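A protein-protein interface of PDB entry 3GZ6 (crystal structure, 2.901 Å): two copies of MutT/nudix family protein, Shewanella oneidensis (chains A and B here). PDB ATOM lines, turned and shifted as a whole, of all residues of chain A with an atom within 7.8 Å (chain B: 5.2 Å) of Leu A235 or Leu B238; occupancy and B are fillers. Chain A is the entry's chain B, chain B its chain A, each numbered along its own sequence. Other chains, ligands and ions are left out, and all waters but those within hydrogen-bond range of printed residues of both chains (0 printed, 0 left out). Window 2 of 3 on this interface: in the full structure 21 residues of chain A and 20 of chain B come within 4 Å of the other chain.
Among the printed residues, pairs that only touch across the chains: Phe A234 with Asn B237, Leu A235 with Arg B236, Leu A235 with Leu B238 and Arg A236 with Leu B235.
Leu A235 touches Arg B236, and with the chains exchanged Arg A236 touches Leu B235.
Leu A235 touches Asn B237, and with the chains exchanged Asn A237 touches Leu B235.
Leu A235 touches Leu B238, but with the chains exchanged Leu A238 does not touch Leu B235 (4.6 Å).
Positions printed for both chains: 161, 199, 235, 236, 237 and 238.
Of the 6 pairs that touch across the chains among the printed residues, 4 have their exchanged pair printed and touching as well.
N of Asn A237 sits at hydrogen-bond distance from O of Leu B235.
N of Asn B237 is in hydrogen-bond range of O of Leu A235, at 2.8 Å.
N of Leu B238 is in hydrogen-bond range of O of Leu B161, at 3.1 Å.
The guanidinium group (NH1) of Arg B199 is in hydrogen-bond range of the backbone carbonyl oxygen (O) of Arg B236, at 2.8 Å.
The side-chain carboxylate (OE2) of Glu B239 is in salt-bridge range of the guanidinium group (NH2) of Arg B236.
The backbone carbonyl oxygen (O) of Tyr A162 sits at hydrogen-bond distance from the backbone NH (N) of Phe A234, at 2.8 Å.
The guanidinium group (NH1) of Arg A199 is in hydrogen-bond range of the backbone carbonyl oxygen (O) of Arg A236 (3.1 Å).
Printed residues of chain B within 4 Å of Phe A234: Asn B237 (3.9 Å).
Leu A235 touches just these residues of chain B: Arg B236 (3.8 Å), Asn B237 (2.8 Å) and Leu B238 (3.9 Å).
Of the printed residues of chain B, Arg A236 touches Leu B235 (3.8 Å).
Printed residues of chain A within 4 Å of Leu B235: Arg A236 (3.8 Å) and Asn A237 (2.9 Å).
Of the printed residues of chain A, Arg B236 touches Leu A235 (3.8 Å).
Of the printed residues of chain A, Asn B237 touches Phe A234 and Leu A235.
The nearest residue of chain A that does not touch Leu B238 is Arg A236 (7.7 Å).
Of the 11 printed residues of chain A, 4 touch a printed residue of chain B.
Of the 12 printed residues of chain B, 4 touch a printed residue of chain A.
Among the printed residues, 6 pairs touch across the chains.
Among the printed residues, no Asp or Glu carboxylate lies within 4 Å of a Lys or Arg side-chain nitrogen of the other chain.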
ATOM      1  N   LEU A 161      33.078  11.247 -21.733  1.00  0.00           N
ATOM      2  CA  LEU A 161      31.789  10.702 -22.183  1.00  0.00           C
ATOM      3  C   LEU A 161      30.791  10.385 -21.072  1.00  0.00           C
ATOM      4  O   LEU A 161      29.581  10.405 -21.306  1.00  0.00           O
ATOM      5  CB  LEU A 161      31.987   9.438 -23.011  1.00  0.00           C
ATOM      6  CG  LEU A 161      32.942   9.541 -24.188  1.00  0.00           C
ATOM      7  CD1 LEU A 161      33.179   8.156 -24.756  1.00  0.00           C
ATOM      8  CD2 LEU A 161      32.358  10.467 -25.221  1.00  0.00           C
ATOM      9  N   TYR A 162      31.282  10.083 -19.871  1.00  0.00           N
ATOM     10  CA  TYR A 162      30.379   9.633 -18.820  1.00  0.00           C
ATOM     11  C   TYR A 162      30.620  10.172 -17.394  1.00  0.00           C
ATOM     12  O   TYR A 162      30.107   9.618 -16.428  1.00  0.00           O
ATOM     13  CB  TYR A 162      30.308   8.106 -18.830  1.00  0.00           C
ATOM     14  CG  TYR A 162      31.640   7.420 -18.621  1.00  0.00           C
ATOM     15  CD1 TYR A 162      32.231   6.653 -19.634  1.00  0.00           C
ATOM     16  CD2 TYR A 162      32.300   7.514 -17.399  1.00  0.00           C
ATOM     17  CE1 TYR A 162      33.464   6.004 -19.423  1.00  0.00           C
ATOM     18  CE2 TYR A 162      33.518   6.881 -17.179  1.00  0.00           C
ATOM     19  CZ  TYR A 162      34.097   6.131 -18.183  1.00  0.00           C
ATOM     20  OH  TYR A 162      35.308   5.523 -17.914  1.00  0.00           O
ATOM     21  N   ARG A 199      22.380  17.175 -18.663  1.00  0.00           N
ATOM     22  CA  ARG A 199      23.156  16.209 -17.898  1.00  0.00           C
ATOM     23  C   ARG A 199      23.670  16.784 -16.587  1.00  0.00           C
ATOM     24  O   ARG A 199      23.515  16.196 -15.516  1.00  0.00           O
ATOM     25  CB  ARG A 199      24.320  15.694 -18.743  1.00  0.00           C
ATOM     26  CG  ARG A 199      23.905  14.649 -19.762  1.00  0.00           C
ATOM     27  CD  ARG A 199      24.975  14.419 -20.775  1.00  0.00           C
ATOM     28  NE  ARG A 199      26.083  13.623 -20.272  1.00  0.00           N
ATOM     29  CZ  ARG A 199      26.162  12.310 -20.427  1.00  0.00           C
ATOM     30  NH1 ARG A 199      25.194  11.668 -21.060  1.00  0.00           N
ATOM     31  NH2 ARG A 199      27.205  11.641 -19.959  1.00  0.00           N
ATOM     32  N   GLN A 202      20.911  17.452 -14.002  1.00  0.00           N
ATOM     33  CA  GLN A 202      20.425  16.169 -13.529  1.00  0.00           C
ATOM     34  C   GLN A 202      21.410  15.551 -12.544  1.00  0.00           C
ATOM     35  O   GLN A 202      21.036  15.189 -11.436  1.00  0.00           O
ATOM     36  CB  GLN A 202      20.210  15.235 -14.712  1.00  0.00           C
ATOM     37  CG  GLN A 202      19.049  14.285 -14.550  1.00  0.00           C
ATOM     38  CD  GLN A 202      19.146  13.107 -15.497  1.00  0.00           C
ATOM     39  OE1 GLN A 202      18.198  12.335 -15.635  1.00  0.00           O
ATOM     40  NE2 GLN A 202      20.303  12.960 -16.154  1.00  0.00           N
ATOM     41  N   TYR A 232      31.131  10.037  -9.561  1.00  0.00           N
ATOM     42  CA  TYR A 232      29.850  10.003 -10.264  1.00  0.00           C
ATOM     43  C   TYR A 232      29.959   9.671 -11.740  1.00  0.00           C
ATOM     44  O   TYR A 232      30.724  10.289 -12.480  1.00  0.00           O
ATOM     45  CB  TYR A 232      29.089  11.311 -10.111  1.00  0.00           C
ATOM     46  CG  TYR A 232      27.770  11.296 -10.838  1.00  0.00           C
ATOM     47  CD1 TYR A 232      26.578  11.146 -10.151  1.00  0.00           C
ATOM     48  CD2 TYR A 232      27.714  11.422 -12.219  1.00  0.00           C
ATOM     49  CE1 TYR A 232      25.361  11.128 -10.826  1.00  0.00           C
ATOM     50  CE2 TYR A 232      26.502  11.413 -12.902  1.00  0.00           C
ATOM     51  CZ  TYR A 232      25.328  11.264 -12.200  1.00  0.00           C
ATOM     52  OH  TYR A 232      24.118  11.248 -12.868  1.00  0.00           O
ATOM     53  N   ARG A 233      29.141   8.717 -12.165  1.00  0.00           N
ATOM     54  CA  ARG A 233      29.161   8.278 -13.547  1.00  0.00           C
ATOM     55  C   ARG A 233      27.759   8.330 -14.155  1.00  0.00           C
ATOM     56  O   ARG A 233      26.771   7.962 -13.529  1.00  0.00           O
ATOM     57  CB  ARG A 233      29.783   6.877 -13.660  1.00  0.00           C
ATOM     58  CG  ARG A 233      31.224   6.765 -13.100  1.00  0.00           C
ATOM     59  CD  ARG A 233      32.229   7.518 -13.953  1.00  0.00           C
ATOM     60  NE  ARG A 233      33.588   7.561 -13.405  1.00  0.00           N
ATOM     61  CZ  ARG A 233      34.016   8.496 -12.562  1.00  0.00           C
ATOM     62  NH1 ARG A 233      33.187   9.433 -12.142  1.00  0.00           N
ATOM     63  NH2 ARG A 233      35.264   8.490 -12.126  1.00  0.00           N
ATOM     64  N   PHE A 234      27.676   8.816 -15.382  1.00  0.00           N
ATOM     65  CA  PHE A 234      26.390   8.894 -16.036  1.00  0.00           C
ATOM     66  C   PHE A 234      25.962   7.505 -16.490  1.00  0.00           C
ATOM     67  O   PHE A 234      26.809   6.664 -16.799  1.00  0.00           O
ATOM     68  CB  PHE A 234      26.444   9.874 -17.206  1.00  0.00           C
ATOM     69  CG  PHE A 234      26.405  11.312 -16.784  1.00  0.00           C
ATOM     70  CD1 PHE A 234      25.207  11.903 -16.411  1.00  0.00           C
ATOM     71  CD2 PHE A 234      27.562  12.075 -16.752  1.00  0.00           C
ATOM     72  CE1 PHE A 234      25.159  13.224 -16.013  1.00  0.00           C
ATOM     73  CE2 PHE A 234      27.522  13.409 -16.358  1.00  0.00           C
ATOM     74  CZ  PHE A 234      26.317  13.981 -15.987  1.00  0.00           C
ATOM     75  N   LEU A 235      24.651   7.273 -16.508  1.00  0.00           N
ATOM     76  CA  LEU A 235      24.087   5.994 -16.939  1.00  0.00           C
ATOM     77  C   LEU A 235      24.166   5.835 -18.445  1.00  0.00           C
ATOM     78  O   LEU A 235      24.346   4.731 -18.946  1.00  0.00           O
ATOM     79  CB  LEU A 235      22.632   5.832 -16.475  1.00  0.00           C
ATOM     80  CG  LEU A 235      22.494   5.304 -15.040  1.00  0.00           C
ATOM     81  CD1 LEU A 235      21.243   5.847 -14.356  1.00  0.00           C
ATOM     82  CD2 LEU A 235      22.542   3.768 -14.992  1.00  0.00           C
ATOM     83  N   ARG A 236      24.032   6.935 -19.172  1.00  0.00           N
ATOM     84  CA  ARG A 236      24.237   6.882 -20.607  1.00  0.00           C
ATOM     85  C   ARG A 236      25.451   7.715 -21.004  1.00  0.00           C
ATOM     86  O   ARG A 236      25.743   8.739 -20.390  1.00  0.00           O
ATOM     87  CB  ARG A 236      22.985   7.331 -21.373  1.00  0.00           C
ATOM     88  CG  ARG A 236      23.216   7.473 -22.878  1.00  0.00           C
ATOM     89  CD  ARG A 236      21.918   7.568 -23.675  1.00  0.00           C
ATOM     90  NE  ARG A 236      22.168   7.989 -25.051  1.00  0.00           N
ATOM     91  CZ  ARG A 236      21.271   7.912 -26.030  1.00  0.00           C
ATOM     92  NH1 ARG A 236      20.060   7.411 -25.789  1.00  0.00           N
ATOM     93  NH2 ARG A 236      21.589   8.330 -27.251  1.00  0.00           N
ATOM     94  N   ASN A 237      26.162   7.253 -22.027  1.00  0.00           N
ATOM     95  CA  ASN A 237      27.279   7.992 -22.593  1.00  0.00           C
ATOM     96  C   ASN A 237      26.744   9.080 -23.520  1.00  0.00           C
ATOM     97  O   ASN A 237      25.609   9.007 -23.993  1.00  0.00           O
ATOM     98  CB  ASN A 237      28.220   7.049 -23.379  1.00  0.00           C
ATOM     99  CG  ASN A 237      29.203   6.255 -22.467  1.00  0.00           C
ATOM    100  OD1 ASN A 237      29.317   6.500 -21.261  1.00  0.00           O
ATOM    101  ND2 ASN A 237      29.920   5.308 -23.063  1.00  0.00           N
ATOM    102  N   LEU A 238      27.549  10.103 -23.768  1.00  0.00           N
ATOM    103  CA  LEU A 238      27.318  10.950 -24.924  1.00  0.00           C
ATOM    104  C   LEU A 238      27.833  10.176 -26.140  1.00  0.00           C
ATOM    105  O   LEU A 238      28.344   9.056 -26.003  1.00  0.00           O
ATOM    106  CB  LEU A 238      28.077  12.269 -24.781  1.00  0.00           C
ATOM    107  CG  LEU A 238      27.719  13.200 -23.623  1.00  0.00           C
ATOM    108  CD1 LEU A 238      28.819  14.224 -23.382  1.00  0.00           C
ATOM    109  CD2 LEU A 238      26.417  13.891 -23.928  1.00  0.00           C
ATOM    110  N   ALA B 160      29.296  -5.901 -16.129  1.00  0.00           N
ATOM    111  CA  ALA B 160      28.010  -6.534 -16.406  1.00  0.00           C
ATOM    112  C   ALA B 160      27.015  -5.513 -16.918  1.00  0.00           C
ATOM    113  O   ALA B 160      26.169  -5.838 -17.745  1.00  0.00           O
ATOM    114  CB  ALA B 160      27.468  -7.223 -15.177  1.00  0.00           C
ATOM    115  N   LEU B 161      27.129  -4.273 -16.446  1.00  0.00           N
ATOM    116  CA  LEU B 161      26.212  -3.200 -16.856  1.00  0.00           C
ATOM    117  C   LEU B 161      26.438  -2.664 -18.270  1.00  0.00           C
ATOM    118  O   LEU B 161      25.517  -2.123 -18.873  1.00  0.00           O
ATOM    119  CB  LEU B 161      26.288  -2.023 -15.894  1.00  0.00           C
ATOM    120  CG  LEU B 161      25.935  -2.273 -14.438  1.00  0.00           C
ATOM    121  CD1 LEU B 161      26.308  -1.044 -13.620  1.00  0.00           C
ATOM    122  CD2 LEU B 161      24.470  -2.568 -14.354  1.00  0.00           C
ATOM    123  N   LEU B 187      24.795  -8.612 -10.858  1.00  0.00           N
ATOM    124  CA  LEU B 187      24.030  -7.445 -10.468  1.00  0.00           C
ATOM    125  C   LEU B 187      23.160  -7.737  -9.266  1.00  0.00           C
ATOM    126  O   LEU B 187      22.493  -6.847  -8.764  1.00  0.00           O
ATOM    127  CB  LEU B 187      23.123  -7.017 -11.597  1.00  0.00           C
ATOM    128  CG  LEU B 187      23.814  -6.631 -12.885  1.00  0.00           C
ATOM    129  CD1 LEU B 187      22.746  -6.101 -13.788  1.00  0.00           C
ATOM    130  CD2 LEU B 187      24.869  -5.586 -12.617  1.00  0.00           C
ATOM    131  N   ILE B 191      17.138  -9.411 -14.582  1.00  0.00           N
ATOM    132  CA  ILE B 191      17.248  -8.497 -15.716  1.00  0.00           C
ATOM    133  C   ILE B 191      16.138  -8.811 -16.694  1.00  0.00           C
ATOM    134  O   ILE B 191      15.774  -9.970 -16.878  1.00  0.00           O
ATOM    135  CB  ILE B 191      18.596  -8.675 -16.479  1.00  0.00           C
ATOM    136  CG1 ILE B 191      19.758  -8.050 -15.728  1.00  0.00           C
ATOM    137  CG2 ILE B 191      18.540  -8.022 -17.831  1.00  0.00           C
ATOM    138  CD1 ILE B 191      21.099  -8.582 -16.183  1.00  0.00           C
ATOM    139  N   SER B 195      15.312  -6.843 -22.881  1.00  0.00           N
ATOM    140  CA  SER B 195      16.344  -5.804 -22.910  1.00  0.00           C
ATOM    141  C   SER B 195      17.675  -6.405 -23.293  1.00  0.00           C
ATOM    142  O   SER B 195      18.373  -5.894 -24.168  1.00  0.00           O
ATOM    143  CB  SER B 195      16.490  -5.148 -21.540  1.00  0.00           C
ATOM    144  OG  SER B 195      15.408  -4.277 -21.263  1.00  0.00           O
ATOM    145  N   PHE B 196      18.016  -7.497 -22.617  1.00  0.00           N
ATOM    146  CA  PHE B 196      19.284  -8.183 -22.817  1.00  0.00           C
ATOM    147  C   PHE B 196      19.399  -8.662 -24.246  1.00  0.00           C
ATOM    148  O   PHE B 196      20.411  -8.445 -24.914  1.00  0.00           O
ATOM    149  CB  PHE B 196      19.376  -9.375 -21.879  1.00  0.00           C
ATOM    150  CG  PHE B 196      20.772  -9.851 -21.631  1.00  0.00           C
ATOM    151  CD1 PHE B 196      21.683  -9.049 -20.975  1.00  0.00           C
ATOM    152  CD2 PHE B 196      21.164 -11.120 -22.015  1.00  0.00           C
ATOM    153  CE1 PHE B 196      22.971  -9.495 -20.727  1.00  0.00           C
ATOM    154  CE2 PHE B 196      22.451 -11.567 -21.778  1.00  0.00           C
ATOM    155  CZ  PHE B 196      23.356 -10.756 -21.130  1.00  0.00           C
ATOM    156  N   ARG B 199      20.025  -5.774 -26.677  1.00  0.00           N
ATOM    157  CA  ARG B 199      21.404  -5.333 -26.553  1.00  0.00           C
ATOM    158  C   ARG B 199      22.377  -6.270 -27.258  1.00  0.00           C
ATOM    159  O   ARG B 199      23.214  -5.854 -28.065  1.00  0.00           O
ATOM    160  CB  ARG B 199      21.772  -5.207 -25.072  1.00  0.00           C
ATOM    161  CG  ARG B 199      21.327  -3.899 -24.444  1.00  0.00           C
ATOM    162  CD  ARG B 199      21.437  -3.931 -22.953  1.00  0.00           C
ATOM    163  NE  ARG B 199      22.803  -3.775 -22.470  1.00  0.00           N
ATOM    164  CZ  ARG B 199      23.345  -2.603 -22.158  1.00  0.00           C
ATOM    165  NH1 ARG B 199      22.633  -1.493 -22.287  1.00  0.00           N
ATOM    166  NH2 ARG B 199      24.589  -2.541 -21.715  1.00  0.00           N
ATOM    167  N   LEU B 235      26.777   1.918 -25.204  1.00  0.00           N
ATOM    168  CA  LEU B 235      26.598   3.362 -25.015  1.00  0.00           C
ATOM    169  C   LEU B 235      25.802   3.653 -23.765  1.00  0.00           C
ATOM    170  O   LEU B 235      26.126   4.569 -23.019  1.00  0.00           O
ATOM    171  CB  LEU B 235      25.871   4.013 -26.194  1.00  0.00           C
ATOM    172  CG  LEU B 235      26.614   4.125 -27.525  1.00  0.00           C
ATOM    173  CD1 LEU B 235      25.821   5.009 -28.486  1.00  0.00           C
ATOM    174  CD2 LEU B 235      28.031   4.653 -27.318  1.00  0.00           C
ATOM    175  N   ARG B 236      24.743   2.882 -23.547  1.00  0.00           N
ATOM    176  CA  ARG B 236      23.941   3.061 -22.354  1.00  0.00           C
ATOM    177  C   ARG B 236      24.142   1.886 -21.409  1.00  0.00           C
ATOM    178  O   ARG B 236      24.268   0.742 -21.843  1.00  0.00           O
ATOM    179  CB  ARG B 236      22.454   3.260 -22.701  1.00  0.00           C
ATOM    180  CG  ARG B 236      21.521   3.274 -21.473  1.00  0.00           C
ATOM    181  CD  ARG B 236      20.172   3.953 -21.752  1.00  0.00           C
ATOM    182  NE  ARG B 236      19.192   3.703 -20.692  1.00  0.00           N
ATOM    183  CZ  ARG B 236      17.996   4.286 -20.623  1.00  0.00           C
ATOM    184  NH1 ARG B 236      17.627   5.172 -21.546  1.00  0.00           N
ATOM    185  NH2 ARG B 236      17.165   3.986 -19.627  1.00  0.00           N
ATOM    186  N   ASN B 237      24.190   2.191 -20.114  1.00  0.00           N
ATOM    187  CA  ASN B 237      24.189   1.183 -19.056  1.00  0.00           C
ATOM    188  C   ASN B 237      22.801   0.556 -18.920  1.00  0.00           C
ATOM    189  O   ASN B 237      21.784   1.214 -19.158  1.00  0.00           O
ATOM    190  CB  ASN B 237      24.590   1.807 -17.695  1.00  0.00           C
ATOM    191  CG  ASN B 237      26.123   2.015 -17.536  1.00  0.00           C
ATOM    192  OD1 ASN B 237      26.940   1.518 -18.320  1.00  0.00           O
ATOM    193  ND2 ASN B 237      26.503   2.748 -16.497  1.00  0.00           N
ATOM    194  N   LEU B 238      22.750  -0.715 -18.541  1.00  0.00           N
ATOM    195  CA  LEU B 238      21.526  -1.244 -17.961  1.00  0.00           C
ATOM    196  C   LEU B 238      21.374  -0.577 -16.596  1.00  0.00           C
ATOM    197  O   LEU B 238      22.313   0.053 -16.090  1.00  0.00           O
ATOM    198  CB  LEU B 238      21.621  -2.756 -17.771  1.00  0.00           C
ATOM    199  CG  LEU B 238      21.747  -3.686 -18.973  1.00  0.00           C
ATOM    200  CD1 LEU B 238      22.096  -5.097 -18.505  1.00  0.00           C
ATOM    201  CD2 LEU B 238      20.454  -3.690 -19.734  1.00  0.00           C
ATOM    202  N   GLU B 239      20.200  -0.724 -15.995  1.00  0.00           N
ATOM    203  CA  GLU B 239      19.976  -0.248 -14.632  1.00  0.00           C
ATOM    204  C   GLU B 239      19.986  -1.393 -13.612  1.00  0.00           C
ATOM    205  O   GLU B 239      20.717  -1.345 -12.612  1.00  0.00           O
ATOM    206  CB  GLU B 239      18.661   0.520 -14.558  1.00  0.00           C
ATOM    207  CG  GLU B 239      18.590   1.684 -15.540  1.00  0.00           C
ATOM    208  CD  GLU B 239      17.174   1.968 -16.020  1.00  0.00           C
ATOM    209  OE1 GLU B 239      16.205   1.628 -15.297  1.00  0.00           O
ATOM    210  OE2 GLU B 239      17.035   2.530 -17.131  1.00  0.00           O
